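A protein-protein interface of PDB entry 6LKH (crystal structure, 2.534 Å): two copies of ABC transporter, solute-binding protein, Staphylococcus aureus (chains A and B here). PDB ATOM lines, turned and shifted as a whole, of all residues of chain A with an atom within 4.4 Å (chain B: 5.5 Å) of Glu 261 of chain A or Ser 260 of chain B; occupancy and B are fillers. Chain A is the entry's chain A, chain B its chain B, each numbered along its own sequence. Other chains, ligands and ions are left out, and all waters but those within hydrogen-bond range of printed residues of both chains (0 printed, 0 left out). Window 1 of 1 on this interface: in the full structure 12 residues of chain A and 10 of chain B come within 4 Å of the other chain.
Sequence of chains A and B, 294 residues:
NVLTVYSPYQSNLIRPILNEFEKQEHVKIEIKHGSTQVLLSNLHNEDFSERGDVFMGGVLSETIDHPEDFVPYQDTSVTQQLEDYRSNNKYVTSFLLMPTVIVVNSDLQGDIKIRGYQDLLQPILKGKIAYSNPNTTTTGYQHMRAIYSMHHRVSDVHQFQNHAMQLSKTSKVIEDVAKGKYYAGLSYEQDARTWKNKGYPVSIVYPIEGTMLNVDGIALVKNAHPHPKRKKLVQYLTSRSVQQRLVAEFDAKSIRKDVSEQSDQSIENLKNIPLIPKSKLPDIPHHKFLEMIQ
Ser 260 of chain A touches Glu 261 of chain B, and with the chains exchanged Glu 261 of chain A touches Ser 260 of chain B.
Ser 260 of chain A touches Gln 262 of chain B, and with the chains exchanged Gln 262 of chain A touches Ser 260 of chain B.
Glu 261 of chain A touches its own counterpart, Glu 261 of chain B.
Ser 263 of chain A touches Ser 260 of chain B, but with the chains exchanged Ser 260 of chain A does not touch Ser 263 of chain B (4.4 Å).
Of the 9 pairs that touch across the chains among the printed residues, 5 have their exchanged pair printed and touching as well.
The side-chain amide nitrogen of Gln 262 of chain A sits close to the backbone carbonyl oxygen of Val 247 of chain A, 3.4 Å away.
The backbone NH (N) of Leu 270 of chain A lies within hydrogen-bond range of the side-chain carboxylate (OE1) of Glu 261 of chain A, 3.1 Å away.
Along chain A the printed residues that touch a printed residue of chain B span positions 260 to 269.
Among the printed residues, 9 pairs touch across the chains.
The backbone carbonyl oxygen (O) of Glu 261 of chain B lies within hydrogen-bond range of the side-chain hydroxyl (OG) of Ser 260 of chain A (3.2 Å).
N of Ser 263 of chain A sits at hydrogen-bond distance from OG of Ser 260 of chain B (3.2 Å).
O of Glu 261 of chain A sits close to O of Glu 261 of chain B, 3.4 Å away.
The side-chain amide nitrogen (ND2) of Asn 269 of chain A lies close to the backbone carbonyl oxygen (O) of Lys 257 of chain B (2.3 Å).
Among the printed residues, pairs that only touch across the chains: Ser 260 of chain A with Gln 262 of chain B (3.6 Å), Glu 261 of chain A with Ser 260 of chain B (3.9 Å), Gln 262 of chain A with Ser 260 of chain B (3.5 Å), Asn 269 of chain A with Asp 258 of chain B (3.6 Å) and Asn 269 of chain A with Val 259 of chain B (3.8 Å).
Of the printed residues of chain B, Glu 261 of chain A touches Ser 260 (3.9 Å) and Glu 261 (3.4 Å).
Printed residues of chain B within 4 Å of Asn 269 of chain A: Lys 257 (2.3 Å), Asp 258 (3.6 Å) and Val 259 (3.8 Å).
Ser 260 of chain B touches just these residues of chain A: Glu 261 (3.9 Å), Gln 262 (3.5 Å) and Ser 263 (3.2 Å).
Of the printed residues of chain A, Glu 261 of chain B touches Ser 260 and Glu 261.
Of the printed residues of chain A, Gln 262 of chain B touches Ser 260 (3.6 Å).
The nearest residue of chain B that does not touch Glu 261 of chain A is Ser 263 of chain B (4.9 Å).
The nearest residue of chain A that does not touch Ser 260 of chain B is Asn 269 of chain A (4.2 Å).
The nearest printed residue of chain A that does not touch Lys 257 of chain B is Leu 270 of chain A (6.3 Å).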
ATOM      1  N   VAL A 247     -25.093  18.326  20.503  1.00  0.00           N
ATOM      2  CA  VAL A 247     -24.642  17.338  19.563  1.00  0.00           C
ATOM      3  C   VAL A 247     -24.683  15.949  20.077  1.00  0.00           C
ATOM      4  O   VAL A 247     -25.023  15.053  19.395  1.00  0.00           O
ATOM      5  CB  VAL A 247     -23.276  17.659  19.087  1.00  0.00           C
ATOM      6  CG1 VAL A 247     -22.722  16.658  18.148  1.00  0.00           C
ATOM      7  CG2 VAL A 247     -23.373  18.894  18.348  1.00  0.00           C
ATOM      8  N   LYS A 253     -27.051  19.721  14.920  1.00  0.00           N
ATOM      9  CA  LYS A 253     -25.920  20.154  14.110  1.00  0.00           C
ATOM     10  C   LYS A 253     -25.437  21.504  14.620  1.00  0.00           C
ATOM     11  O   LYS A 253     -26.185  22.487  14.599  1.00  0.00           O
ATOM     12  CB  LYS A 253     -26.308  20.224  12.635  1.00  0.00           C
ATOM     13  CG  LYS A 253     -26.584  18.859  12.049  1.00  0.00           C
ATOM     14  CD  LYS A 253     -27.089  18.941  10.634  1.00  0.00           C
ATOM     15  CE  LYS A 253     -26.999  17.591   9.957  1.00  0.00           C
ATOM     16  NZ  LYS A 253     -27.600  16.507  10.790  1.00  0.00           N
ATOM     17  N   VAL A 259     -16.764  22.140  16.933  1.00  0.00           N
ATOM     18  CA  VAL A 259     -17.635  21.098  17.466  1.00  0.00           C
ATOM     19  C   VAL A 259     -17.914  20.103  16.349  1.00  0.00           C
ATOM     20  O   VAL A 259     -18.588  20.437  15.366  1.00  0.00           O
ATOM     21  CB  VAL A 259     -18.943  21.678  18.020  1.00  0.00           C
ATOM     22  CG1 VAL A 259     -19.890  20.563  18.439  1.00  0.00           C
ATOM     23  CG2 VAL A 259     -18.650  22.595  19.191  1.00  0.00           C
ATOM     24  N   SER A 260     -17.551  18.904  16.534  1.00  0.00           N
ATOM     25  CA  SER A 260     -17.694  17.973  15.494  1.00  0.00           C
ATOM     26  C   SER A 260     -19.079  17.420  15.402  1.00  0.00           C
ATOM     27  O   SER A 260     -19.844  17.556  16.238  1.00  0.00           O
ATOM     28  CB  SER A 260     -16.632  16.909  15.687  1.00  0.00           C
ATOM     29  OG  SER A 260     -17.015  15.707  15.151  1.00  0.00           O
ATOM     30  N   GLU A 261     -19.372  16.784  14.325  1.00  0.00           N
ATOM     31  CA  GLU A 261     -20.641  16.154  14.186  1.00  0.00           C
ATOM     32  C   GLU A 261     -20.619  14.824  14.836  1.00  0.00           C
ATOM     33  O   GLU A 261     -19.652  14.435  15.348  1.00  0.00           O
ATOM     34  CB  GLU A 261     -21.009  16.030  12.728  1.00  0.00           C
ATOM     35  CG  GLU A 261     -21.739  17.237  12.258  1.00  0.00           C
ATOM     36  CD  GLU A 261     -22.306  17.216  10.845  1.00  0.00           C
ATOM     37  OE1 GLU A 261     -23.345  16.615  10.554  1.00  0.00           O
ATOM     38  OE2 GLU A 261     -21.728  17.908  10.023  1.00  0.00           O
ATOM     39  N   GLN A 262     -21.711  14.123  14.813  1.00  0.00           N
ATOM     40  CA  GLN A 262     -21.855  12.884  15.520  1.00  0.00           C
ATOM     41  C   GLN A 262     -22.333  11.793  14.645  1.00  0.00           C
ATOM     42  O   GLN A 262     -23.243  12.003  13.949  1.00  0.00           O
ATOM     43  CB  GLN A 262     -22.875  13.085  16.594  1.00  0.00           C
ATOM     44  CG  GLN A 262     -22.675  12.263  17.828  1.00  0.00           C
ATOM     45  CD  GLN A 262     -23.980  12.026  18.532  1.00  0.00           C
ATOM     46  OE1 GLN A 262     -25.019  11.946  17.910  1.00  0.00           O
ATOM     47  NE2 GLN A 262     -23.932  11.897  19.818  1.00  0.00           N
ATOM     48  N   SER A 263     -21.696  10.629  14.702  1.00  0.00           N
ATOM     49  CA  SER A 263     -22.094   9.495  13.878  1.00  0.00           C
ATOM     50  C   SER A 263     -23.396   8.887  14.391  1.00  0.00           C
ATOM     51  O   SER A 263     -23.385   8.001  15.246  1.00  0.00           O
ATOM     52  CB  SER A 263     -20.994   8.433  13.867  1.00  0.00           C
ATOM     53  OG  SER A 263     -20.755   7.933  15.171  1.00  0.00           O
ATOM     54  N   ASN A 269     -24.958  13.363   8.050  1.00  0.00           N
ATOM     55  CA  ASN A 269     -24.073  14.485   8.300  1.00  0.00           C
ATOM     56  C   ASN A 269     -24.213  15.510   7.174  1.00  0.00           C
ATOM     57  O   ASN A 269     -24.652  15.198   6.064  1.00  0.00           O
ATOM     58  CB  ASN A 269     -22.623  14.007   8.436  1.00  0.00           C
ATOM     59  CG  ASN A 269     -22.235  12.999   7.375  1.00  0.00           C
ATOM     60  OD1 ASN A 269     -22.981  12.058   7.095  1.00  0.00           O
ATOM     61  ND2 ASN A 269     -21.068  13.190   6.777  1.00  0.00           N
ATOM     62  N   LEU A 270     -23.847  16.756   7.479  1.00  0.00           N
ATOM     63  CA  LEU A 270     -24.133  17.855   6.559  1.00  0.00           C
ATOM     64  C   LEU A 270     -23.514  17.622   5.185  1.00  0.00           C
ATOM     65  O   LEU A 270     -24.131  17.930   4.159  1.00  0.00           O
ATOM     66  CB  LEU A 270     -23.639  19.175   7.151  1.00  0.00           C
ATOM     67  CG  LEU A 270     -24.714  19.995   7.864  1.00  0.00           C
ATOM     68  CD1 LEU A 270     -24.095  21.131   8.658  1.00  0.00           C
ATOM     69  CD2 LEU A 270     -25.728  20.541   6.871  1.00  0.00           C
ATOM     70  N   VAL B 247     -12.002   6.265  12.073  1.00  0.00           N
ATOM     71  CA  VAL B 247     -12.425   7.389  12.810  1.00  0.00           C
ATOM     72  C   VAL B 247     -12.580   7.060  14.245  1.00  0.00           C
ATOM     73  O   VAL B 247     -11.970   7.645  15.070  1.00  0.00           O
ATOM     74  CB  VAL B 247     -13.689   7.969  12.260  1.00  0.00           C
ATOM     75  CG1 VAL B 247     -14.227   9.069  13.082  1.00  0.00           C
ATOM     76  CG2 VAL B 247     -13.413   8.455  10.907  1.00  0.00           C
ATOM     77  N   LYS B 257     -17.859  11.338   2.359  1.00  0.00           N
ATOM     78  CA  LYS B 257     -18.875  12.299   2.782  1.00  0.00           C
ATOM     79  C   LYS B 257     -19.606  11.800   4.019  1.00  0.00           C
ATOM     80  O   LYS B 257     -19.803  12.544   4.985  1.00  0.00           O
ATOM     81  CB  LYS B 257     -19.895  12.537   1.665  1.00  0.00           C
ATOM     82  CG  LYS B 257     -19.355  12.978   0.326  1.00  0.00           C
ATOM     83  CD  LYS B 257     -20.361  12.618  -0.770  1.00  0.00           C
ATOM     84  CE  LYS B 257     -20.723  13.806  -1.648  1.00  0.00           C
ATOM     85  NZ  LYS B 257     -21.838  13.460  -2.579  1.00  0.00           N
ATOM     86  N   ASP B 258     -20.022  10.534   3.997  1.00  0.00           N
ATOM     87  CA  ASP B 258     -20.993   9.990   4.935  1.00  0.00           C
ATOM     88  C   ASP B 258     -20.366   9.483   6.233  1.00  0.00           C
ATOM     89  O   ASP B 258     -20.997   8.693   6.944  1.00  0.00           O
ATOM     90  CB  ASP B 258     -21.779   8.865   4.259  1.00  0.00           C
ATOM     91  CG  ASP B 258     -20.877   7.810   3.641  1.00  0.00           C
ATOM     92  OD1 ASP B 258     -19.651   7.861   3.875  1.00  0.00           O
ATOM     93  OD2 ASP B 258     -21.393   6.935   2.912  1.00  0.00           O
ATOM     94  N   VAL B 259     -19.154   9.916   6.563  1.00  0.00           N
ATOM     95  CA  VAL B 259     -18.491   9.546   7.810  1.00  0.00           C
ATOM     96  C   VAL B 259     -18.142  10.837   8.537  1.00  0.00           C
ATOM     97  O   VAL B 259     -17.259  11.586   8.098  1.00  0.00           O
ATOM     98  CB  VAL B 259     -17.242   8.689   7.569  1.00  0.00           C
ATOM     99  CG1 VAL B 259     -16.534   8.391   8.886  1.00  0.00           C
ATOM    100  CG2 VAL B 259     -17.615   7.399   6.855  1.00  0.00           C
ATOM    101  N   SER B 260     -18.832  11.098   9.643  1.00  0.00           N
ATOM    102  CA  SER B 260     -18.581  12.300  10.422  1.00  0.00           C
ATOM    103  C   SER B 260     -17.252  12.186  11.161  1.00  0.00           C
ATOM    104  O   SER B 260     -16.712  11.096  11.359  1.00  0.00           O
ATOM    105  CB  SER B 260     -19.716  12.540  11.418  1.00  0.00           C
ATOM    106  OG  SER B 260     -20.177  11.320  11.973  1.00  0.00           O
ATOM    107  N   GLU B 261     -16.717  13.338  11.560  1.00  0.00           N
ATOM    108  CA  GLU B 261     -15.496  13.364  12.348  1.00  0.00           C
ATOM    109  C   GLU B 261     -15.804  12.963  13.791  1.00  0.00           C
ATOM    110  O   GLU B 261     -16.953  12.712  14.164  1.00  0.00           O
ATOM    111  CB  GLU B 261     -14.847  14.744  12.292  1.00  0.00           C
ATOM    112  CG  GLU B 261     -14.708  15.314  10.887  1.00  0.00           C
ATOM    113  CD  GLU B 261     -13.387  16.030  10.661  1.00  0.00           C
ATOM    114  OE1 GLU B 261     -12.713  16.382  11.651  1.00  0.00           O
ATOM    115  OE2 GLU B 261     -13.018  16.236   9.487  1.00  0.00           O
ATOM    116  N   GLN B 262     -14.761  12.904  14.615  1.00  0.00           N
ATOM    117  CA  GLN B 262     -14.894  12.559  16.023  1.00  0.00           C
ATOM    118  C   GLN B 262     -14.414  13.721  16.889  1.00  0.00           C
ATOM    119  O   GLN B 262     -13.797  14.675  16.407  1.00  0.00           O
ATOM    120  CB  GLN B 262     -14.119  11.277  16.343  1.00  0.00           C
ATOM    121  CG  GLN B 262     -14.845  10.356  17.304  1.00  0.00           C
ATOM    122  CD  GLN B 262     -13.909   9.401  18.001  1.00  0.00           C
ATOM    123  OE1 GLN B 262     -12.702   9.632  18.055  1.00  0.00           O
ATOM    124  NE2 GLN B 262     -14.455   8.316  18.535  1.00  0.00           N
ATOM    125  N   SER B 263     -14.673  13.613  18.195  1.00  0.00           N
ATOM    126  CA  SER B 263     -14.694  14.767  19.090  1.00  0.00           C
ATOM    127  C   SER B 263     -13.386  14.980  19.864  1.00  0.00           C
ATOM    128  O   SER B 263     -13.069  14.222  20.787  1.00  0.00           O
ATOM    129  CB  SER B 263     -15.833  14.619  20.104  1.00  0.00           C
ATOM    130  OG  SER B 263     -17.009  14.119  19.479  1.00  0.00           O
